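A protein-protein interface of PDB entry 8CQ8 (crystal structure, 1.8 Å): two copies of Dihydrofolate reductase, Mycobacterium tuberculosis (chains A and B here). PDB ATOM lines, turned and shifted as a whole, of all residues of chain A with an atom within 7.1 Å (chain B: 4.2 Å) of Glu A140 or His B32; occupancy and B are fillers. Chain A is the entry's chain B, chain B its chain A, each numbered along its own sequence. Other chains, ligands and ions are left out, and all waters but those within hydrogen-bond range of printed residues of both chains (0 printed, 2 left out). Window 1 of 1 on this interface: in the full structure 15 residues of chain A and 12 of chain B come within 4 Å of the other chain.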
ATOM      1  N   TRP A 137      18.378  18.461  11.823  1.00  0.00           N
ATOM      2  CA  TRP A 137      18.224  19.692  12.580  1.00  0.00           C
ATOM      3  C   TRP A 137      17.678  20.746  11.638  1.00  0.00           C
ATOM      4  O   TRP A 137      18.392  21.208  10.741  1.00  0.00           O
ATOM      5  CB  TRP A 137      19.561  20.123  13.178  1.00  0.00           C
ATOM      6  CG  TRP A 137      19.887  19.284  14.339  1.00  0.00           C
ATOM      7  CD1 TRP A 137      20.659  18.166  14.347  1.00  0.00           C
ATOM      8  CD2 TRP A 137      19.455  19.490  15.687  1.00  0.00           C
ATOM      9  NE1 TRP A 137      20.715  17.641  15.616  1.00  0.00           N
ATOM     10  CE2 TRP A 137      19.989  18.443  16.458  1.00  0.00           C
ATOM     11  CE3 TRP A 137      18.666  20.462  16.318  1.00  0.00           C
ATOM     12  CZ2 TRP A 137      19.757  18.334  17.823  1.00  0.00           C
ATOM     13  CZ3 TRP A 137      18.443  20.352  17.680  1.00  0.00           C
ATOM     14  CH2 TRP A 137      18.989  19.297  18.416  1.00  0.00           C
ATOM     15  N   ARG A 138      16.404  21.094  11.818  1.00  0.00           N
ATOM     16  CA  ARG A 138      15.785  22.151  11.037  1.00  0.00           C
ATOM     17  C   ARG A 138      16.214  23.478  11.629  1.00  0.00           C
ATOM     18  O   ARG A 138      15.920  23.783  12.790  1.00  0.00           O
ATOM     19  CB  ARG A 138      14.267  22.014  11.009  1.00  0.00           C
ATOM     20  CG  ARG A 138      13.804  21.235   9.805  1.00  0.00           C
ATOM     21  CD  ARG A 138      14.200  19.780   9.930  1.00  0.00           C
ATOM     22  NE  ARG A 138      13.219  18.913   9.289  1.00  0.00           N
ATOM     23  CZ  ARG A 138      13.481  17.698   8.811  1.00  0.00           C
ATOM     24  NH1 ARG A 138      12.516  16.992   8.232  1.00  0.00           N
ATOM     25  NH2 ARG A 138      14.702  17.180   8.918  1.00  0.00           N
ATOM     26  N   GLY A 139      16.949  24.241  10.848  1.00  0.00           N
ATOM     27  CA  GLY A 139      17.622  25.361  11.439  1.00  0.00           C
ATOM     28  C   GLY A 139      17.292  26.611  10.695  1.00  0.00           C
ATOM     29  O   GLY A 139      17.223  26.613   9.463  1.00  0.00           O
ATOM     30  N   GLU A 140      17.047  27.673  11.427  1.00  0.00           N
ATOM     31  CA  GLU A 140      16.512  28.872  10.818  1.00  0.00           C
ATOM     32  C   GLU A 140      17.581  29.944  10.894  1.00  0.00           C
ATOM     33  O   GLU A 140      17.896  30.468  11.971  1.00  0.00           O
ATOM     34  CB  GLU A 140      15.237  29.354  11.480  1.00  0.00           C
ATOM     35  CG  GLU A 140      14.751  30.588  10.819  1.00  0.00           C
ATOM     36  CD  GLU A 140      13.611  31.192  11.572  1.00  0.00           C
ATOM     37  OE1 GLU A 140      13.060  30.484  12.433  1.00  0.00           O
ATOM     38  OE2 GLU A 140      13.186  32.322  11.231  1.00  0.00           O
ATOM     39  N   THR A 141      18.023  30.330   9.717  1.00  0.00           N
ATOM     40  CA  THR A 141      19.209  31.130   9.501  1.00  0.00           C
ATOM     41  C   THR A 141      18.888  32.606   9.678  1.00  0.00           C
ATOM     42  O   THR A 141      17.992  33.128   9.014  1.00  0.00           O
ATOM     43  CB  THR A 141      19.695  30.858   8.078  1.00  0.00           C
ATOM     44  OG1 THR A 141      20.293  29.555   8.018  1.00  0.00           O
ATOM     45  CG2 THR A 141      20.670  31.915   7.595  1.00  0.00           C
ATOM     46  N   GLY A 142      19.612  33.289  10.559  1.00  0.00           N
ATOM     47  CA  GLY A 142      19.540  34.731  10.623  1.00  0.00           C
ATOM     48  C   GLY A 142      20.391  35.365   9.531  1.00  0.00           C
ATOM     49  O   GLY A 142      20.988  34.688   8.691  1.00  0.00           O
ATOM     50  N   LEU A 155      22.855  34.707  13.766  1.00  0.00           N
ATOM     51  CA  LEU A 155      22.355  33.703  14.698  1.00  0.00           C
ATOM     52  C   LEU A 155      21.628  32.593  13.955  1.00  0.00           C
ATOM     53  O   LEU A 155      21.045  32.821  12.890  1.00  0.00           O
ATOM     54  CB  LEU A 155      21.422  34.327  15.739  1.00  0.00           C
ATOM     55  CG  LEU A 155      22.002  35.544  16.479  1.00  0.00           C
ATOM     56  CD1 LEU A 155      20.967  36.197  17.406  1.00  0.00           C
ATOM     57  CD2 LEU A 155      23.279  35.208  17.253  1.00  0.00           C
ATOM     58  N   TYR A 156      21.703  31.385  14.507  1.00  0.00           N
ATOM     59  CA  TYR A 156      20.942  30.239  14.035  1.00  0.00           C
ATOM     60  C   TYR A 156      20.151  29.632  15.178  1.00  0.00           C
ATOM     61  O   TYR A 156      20.655  29.506  16.297  1.00  0.00           O
ATOM     62  CB  TYR A 156      21.834  29.155  13.457  1.00  0.00           C
ATOM     63  CG  TYR A 156      22.562  29.514  12.196  1.00  0.00           C
ATOM     64  CD1 TYR A 156      23.668  30.357  12.217  1.00  0.00           C
ATOM     65  CD2 TYR A 156      22.177  28.966  10.987  1.00  0.00           C
ATOM     66  CE1 TYR A 156      24.350  30.667  11.059  1.00  0.00           C
ATOM     67  CE2 TYR A 156      22.847  29.261   9.833  1.00  0.00           C
ATOM     68  CZ  TYR A 156      23.935  30.113   9.866  1.00  0.00           C
ATOM     69  OH  TYR A 156      24.618  30.409   8.703  1.00  0.00           O
ATOM     70  N   SER A 157      18.922  29.227  14.879  1.00  0.00           N
ATOM     71  CA  SER A 157      18.090  28.509  15.833  1.00  0.00           C
ATOM     72  C   SER A 157      17.725  27.172  15.206  1.00  0.00           C
ATOM     73  O   SER A 157      17.043  27.123  14.177  1.00  0.00           O
ATOM     74  CB  SER A 157      16.860  29.327  16.212  1.00  0.00           C
ATOM     75  OG  SER A 157      17.255  30.583  16.751  1.00  0.00           O
ATOM     76  N   TYR A 158      18.224  26.097  15.805  1.00  0.00           N
ATOM     77  CA  TYR A 158      18.035  24.737  15.330  1.00  0.00           C
ATOM     78  C   TYR A 158      17.028  24.006  16.200  1.00  0.00           C
ATOM     79  O   TYR A 158      16.912  24.245  17.406  1.00  0.00           O
ATOM     80  CB  TYR A 158      19.374  23.997  15.301  1.00  0.00           C
ATOM     81  CG  TYR A 158      20.220  24.524  14.186  1.00  0.00           C
ATOM     82  CD1 TYR A 158      21.154  25.521  14.404  1.00  0.00           C
ATOM     83  CD2 TYR A 158      20.121  23.984  12.917  1.00  0.00           C
ATOM     84  CE1 TYR A 158      21.922  26.003  13.373  1.00  0.00           C
ATOM     85  CE2 TYR A 158      20.881  24.465  11.874  1.00  0.00           C
ATOM     86  CZ  TYR A 158      21.777  25.471  12.109  1.00  0.00           C
ATOM     87  OH  TYR A 158      22.540  25.933  11.072  1.00  0.00           O
ATOM     88  N   HIS A 159      16.279  23.124  15.560  1.00  0.00           N
ATOM     89  CA  HIS A 159      15.255  22.376  16.251  1.00  0.00           C
ATOM     90  C   HIS A 159      15.062  21.081  15.493  1.00  0.00           C
ATOM     91  O   HIS A 159      15.234  21.029  14.272  1.00  0.00           O
ATOM     92  CB  HIS A 159      13.945  23.171  16.337  1.00  0.00           C
ATOM     93  CG  HIS A 159      12.816  22.398  16.937  1.00  0.00           C
ATOM     94  ND1 HIS A 159      12.028  21.547  16.195  1.00  0.00           N
ATOM     95  CD2 HIS A 159      12.342  22.343  18.203  1.00  0.00           C
ATOM     96  CE1 HIS A 159      11.122  20.993  16.979  1.00  0.00           C
ATOM     97  NE2 HIS A 159      11.282  21.468  18.200  1.00  0.00           N
ATOM     98  N   GLU B  28       4.687  27.418   3.666  1.00  0.00           N
ATOM     99  CA  GLU B  28       5.935  27.601   4.392  1.00  0.00           C
ATOM    100  C   GLU B  28       5.689  27.947   5.851  1.00  0.00           C
ATOM    101  O   GLU B  28       6.424  27.482   6.726  1.00  0.00           O
ATOM    102  CB  GLU B  28       6.752  28.694   3.710  1.00  0.00           C
ATOM    103  CG  GLU B  28       7.066  28.363   2.251  1.00  0.00           C
ATOM    104  CD  GLU B  28       5.938  28.762   1.314  1.00  0.00           C
ATOM    105  OE1 GLU B  28       4.880  29.182   1.817  1.00  0.00           O
ATOM    106  OE2 GLU B  28       6.097  28.666   0.083  1.00  0.00           O
ATOM    107  N   ASP B  29       4.659  28.743   6.141  1.00  0.00           N
ATOM    108  CA  ASP B  29       4.363  29.061   7.532  1.00  0.00           C
ATOM    109  C   ASP B  29       3.697  27.898   8.251  1.00  0.00           C
ATOM    110  O   ASP B  29       3.879  27.731   9.462  1.00  0.00           O
ATOM    111  CB  ASP B  29       3.466  30.285   7.616  1.00  0.00           C
ATOM    112  CG  ASP B  29       3.010  30.554   9.015  1.00  0.00           C
ATOM    113  OD1 ASP B  29       3.859  30.960   9.836  1.00  0.00           O
ATOM    114  OD2 ASP B  29       1.826  30.301   9.317  1.00  0.00           O
ATOM    115  N   GLN B  30       2.928  27.084   7.530  1.00  0.00           N
ATOM    116  CA  GLN B  30       2.313  25.922   8.155  1.00  0.00           C
ATOM    117  C   GLN B  30       3.367  24.909   8.586  1.00  0.00           C
ATOM    118  O   GLN B  30       3.292  24.349   9.689  1.00  0.00           O
ATOM    119  CB  GLN B  30       1.329  25.262   7.201  1.00  0.00           C
ATOM    120  CG  GLN B  30       0.887  23.926   7.735  1.00  0.00           C
ATOM    121  CD  GLN B  30       0.038  23.155   6.762  1.00  0.00           C
ATOM    122  OE1 GLN B  30      -0.158  23.570   5.615  1.00  0.00           O
ATOM    123  NE2 GLN B  30      -0.500  22.033   7.222  1.00  0.00           N
ATOM    124  N   ALA B  31       4.338  24.636   7.711  1.00  0.00           N
ATOM    125  CA  ALA B  31       5.461  23.779   8.084  1.00  0.00           C
ATOM    126  C   ALA B  31       6.204  24.335   9.302  1.00  0.00           C
ATOM    127  O   ALA B  31       6.402  23.632  10.301  1.00  0.00           O
ATOM    128  CB  ALA B  31       6.404  23.627   6.887  1.00  0.00           C
ATOM    129  N   HIS B  32       6.619  25.602   9.228  1.00  0.00           N
ATOM    130  CA  HIS B  32       7.248  26.280  10.362  1.00  0.00           C
ATOM    131  C   HIS B  32       6.455  26.084  11.650  1.00  0.00           C
ATOM    132  O   HIS B  32       7.024  25.823  12.716  1.00  0.00           O
ATOM    133  CB  HIS B  32       7.370  27.763  10.034  1.00  0.00           C
ATOM    134  CG  HIS B  32       7.902  28.605  11.148  1.00  0.00           C
ATOM    135  ND1 HIS B  32       9.190  28.498  11.621  1.00  0.00           N
ATOM    136  CD2 HIS B  32       7.309  29.568  11.890  1.00  0.00           C
ATOM    137  CE1 HIS B  32       9.376  29.374  12.590  1.00  0.00           C
ATOM    138  NE2 HIS B  32       8.244  30.025  12.784  1.00  0.00           N
ATOM    139  N   PHE B  33       5.133  26.232  11.571  1.00  0.00           N
ATOM    140  CA  PHE B  33       4.290  26.076  12.749  1.00  0.00           C
ATOM    141  C   PHE B  33       4.348  24.652  13.278  1.00  0.00           C
ATOM    142  O   PHE B  33       4.540  24.429  14.479  1.00  0.00           O
ATOM    143  CB  PHE B  33       2.856  26.484  12.391  1.00  0.00           C
ATOM    144  CG  PHE B  33       1.829  26.073  13.404  1.00  0.00           C
ATOM    145  CD1 PHE B  33       1.577  26.847  14.530  1.00  0.00           C
ATOM    146  CD2 PHE B  33       1.095  24.908  13.210  1.00  0.00           C
ATOM    147  CE1 PHE B  33       0.625  26.453  15.455  1.00  0.00           C
ATOM    148  CE2 PHE B  33       0.142  24.506  14.128  1.00  0.00           C
ATOM    149  CZ  PHE B  33      -0.097  25.282  15.251  1.00  0.00           C
ATOM    150  N   ARG B  34       4.189  23.669  12.385  1.00  0.00           N
ATOM    151  CA  ARG B  34       4.182  22.269  12.803  1.00  0.00           C
ATOM    152  C   ARG B  34       5.515  21.870  13.413  1.00  0.00           C
ATOM    153  O   ARG B  34       5.559  21.127  14.396  1.00  0.00           O
ATOM    154  CB  ARG B  34       3.860  21.367  11.613  1.00  0.00           C
ATOM    155  CG  ARG B  34       3.849  19.881  11.933  1.00  0.00           C
ATOM    156  CD  ARG B  34       4.038  19.031  10.664  1.00  0.00           C
ATOM    157  NE  ARG B  34       4.000  17.590  10.932  1.00  0.00           N
ATOM    158  CZ  ARG B  34       3.034  16.761  10.537  1.00  0.00           C
ATOM    159  NH1 ARG B  34       2.024  17.215   9.804  1.00  0.00           N
ATOM    160  NH2 ARG B  34       3.093  15.463  10.841  1.00  0.00           N
ATOM    161  N   GLU B  35       6.619  22.353  12.846  1.00  0.00           N
ATOM    162  CA  GLU B  35       7.920  22.038  13.426  1.00  0.00           C
ATOM    163  C   GLU B  35       8.003  22.559  14.862  1.00  0.00           C
ATOM    164  O   GLU B  35       8.445  21.842  15.766  1.00  0.00           O
ATOM    165  CB  GLU B  35       9.044  22.623  12.549  1.00  0.00           C
ATOM    166  CG  GLU B  35      10.498  22.371  13.013  1.00  0.00           C
ATOM    167  CD  GLU B  35      10.984  20.931  12.755  1.00  0.00           C
ATOM    168  OE1 GLU B  35      11.820  20.432  13.550  1.00  0.00           O
ATOM    169  OE2 GLU B  35      10.554  20.314  11.743  1.00  0.00           O
ATOM    170  N   ILE B  36       7.544  23.792  15.101  1.00  0.00           N
ATOM    171  CA  ILE B  36       7.702  24.359  16.436  1.00  0.00           C
ATOM    172  C   ILE B  36       6.719  23.756  17.424  1.00  0.00           C
ATOM    173  O   ILE B  36       7.016  23.654  18.620  1.00  0.00           O
ATOM    174  CB  ILE B  36       7.571  25.886  16.380  1.00  0.00           C
ATOM    175  CG1 ILE B  36       8.655  26.465  15.489  1.00  0.00           C
ATOM    176  CG2 ILE B  36       7.616  26.507  17.780  1.00  0.00           C
ATOM    177  CD1 ILE B  36       8.470  27.909  15.256  1.00  0.00           C
ATOM    178  N   THR B 115       5.544  34.878  12.349  1.00  0.00           N
ATOM    179  CA  THR B 115       5.671  34.947  10.898  1.00  0.00           C
ATOM    180  C   THR B 115       5.081  36.284  10.480  1.00  0.00           C
ATOM    181  O   THR B 115       3.921  36.555  10.769  1.00  0.00           O
ATOM    182  CB  THR B 115       4.928  33.806  10.193  1.00  0.00           C
ATOM    183  OG1 THR B 115       5.357  32.545  10.698  1.00  0.00           O
ATOM    184  CG2 THR B 115       5.203  33.829   8.698  1.00  0.00           C
ATOM    185  N   ARG B 145      11.794  36.304   2.983  1.00  0.00           N
ATOM    186  CA  ARG B 145      11.770  35.081   2.202  1.00  0.00           C
ATOM    187  C   ARG B 145      10.627  35.157   1.196  1.00  0.00           C
ATOM    188  O   ARG B 145       9.788  36.053   1.254  1.00  0.00           O
ATOM    189  CB  ARG B 145      11.630  33.871   3.137  1.00  0.00           C
ATOM    190  CG  ARG B 145      12.730  33.786   4.227  1.00  0.00           C
ATOM    191  CD  ARG B 145      12.333  32.886   5.421  1.00  0.00           C
ATOM    192  NE  ARG B 145      13.341  32.782   6.501  1.00  0.00           N
ATOM    193  CZ  ARG B 145      13.567  33.668   7.484  1.00  0.00           C
ATOM    194  NH1 ARG B 145      12.871  34.802   7.566  1.00  0.00           N
ATOM    195  NH2 ARG B 145      14.514  33.418   8.395  1.00  0.00           N
ATOM    196  N   LEU B 155      10.539  35.579   9.454  1.00  0.00           N
ATOM    197  CA  LEU B 155      10.212  35.064  10.765  1.00  0.00           C
ATOM    198  C   LEU B 155      10.909  35.902  11.826  1.00  0.00           C
ATOM    199  O   LEU B 155      11.968  36.489  11.582  1.00  0.00           O
ATOM    200  CB  LEU B 155      10.589  33.594  10.871  1.00  0.00           C
ATOM    201  CG  LEU B 155      10.104  32.725   9.701  1.00  0.00           C
ATOM    202  CD1 LEU B 155      10.554  31.282   9.768  1.00  0.00           C
ATOM    203  CD2 LEU B 155       8.609  32.741   9.619  1.00  0.00           C
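The side-chain carboxylate (OE2) of Glu B35 lies within salt-bridge range of the guanidinium group (NE) of Arg A138 (3.9 Å).
OE1 of Glu B35 sits at hydrogen-bond distance from ND1 of His A159.
The guanidinium group of Arg B145 lies within salt-bridge range of the side-chain carboxylate of Glu A140 (3.3 Å).
The backbone NH (N) of Arg A138 sits at hydrogen-bond distance from the backbone carbonyl oxygen (O) of His A159 (2.7 Å).
The backbone carbonyl oxygen (O) of Ser A157 is in hydrogen-bond range of the backbone NH (N) of Glu A140 (2.8 Å).
Among the printed residues, merely in contact across the chains: Glu A140 with Leu B155 (2.9 Å), Thr A141 with Arg B145 (3.5 Å) and Glu A140 with His B32 (3.9 Å).
Printed residues of chain B within 4 Å of Arg A138: Glu B35.
Printed residues of chain B within 4 Å of Thr A141: Arg B145.
His B32 touches one residue of chain A.
Printed residues of chain A within 4 Å of Glu B35: Arg A138 and His A159.
Of the printed residues of chain A, Arg B145 touches Glu A140 and Thr A141.
Printed residues of chain A within 4 Å of Leu B155: Glu A140 (2.9 Å).
The nearest printed residue of chain B that does not touch Glu A140 is Ile B36 (6.0 Å).
The nearest printed residue of chain A that does not touch His B32 is His A159 (7.4 Å).
Of the 11 printed residues of chain A, 4 touch a printed residue of chain B.
Hydrophobic or aromatic side chains of chain A within 4 Å of the printed part of chain B: His A159.
Of the 12 printed residues of chain B, 4 touch a printed residue of chain A.
Printed residues of chain B that touch a printed residue of chain A: His B32, Glu B35, Arg B145 and Leu B155.
Among the printed residues, Asp or Glu carboxylates within 4 Å of a Lys or Arg side-chain nitrogen of the other chain: Arg A138 with Glu B35 (3.9 Å) and Glu A140 with Arg B145 (3.3 Å).
Position printed for both chains: 155.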
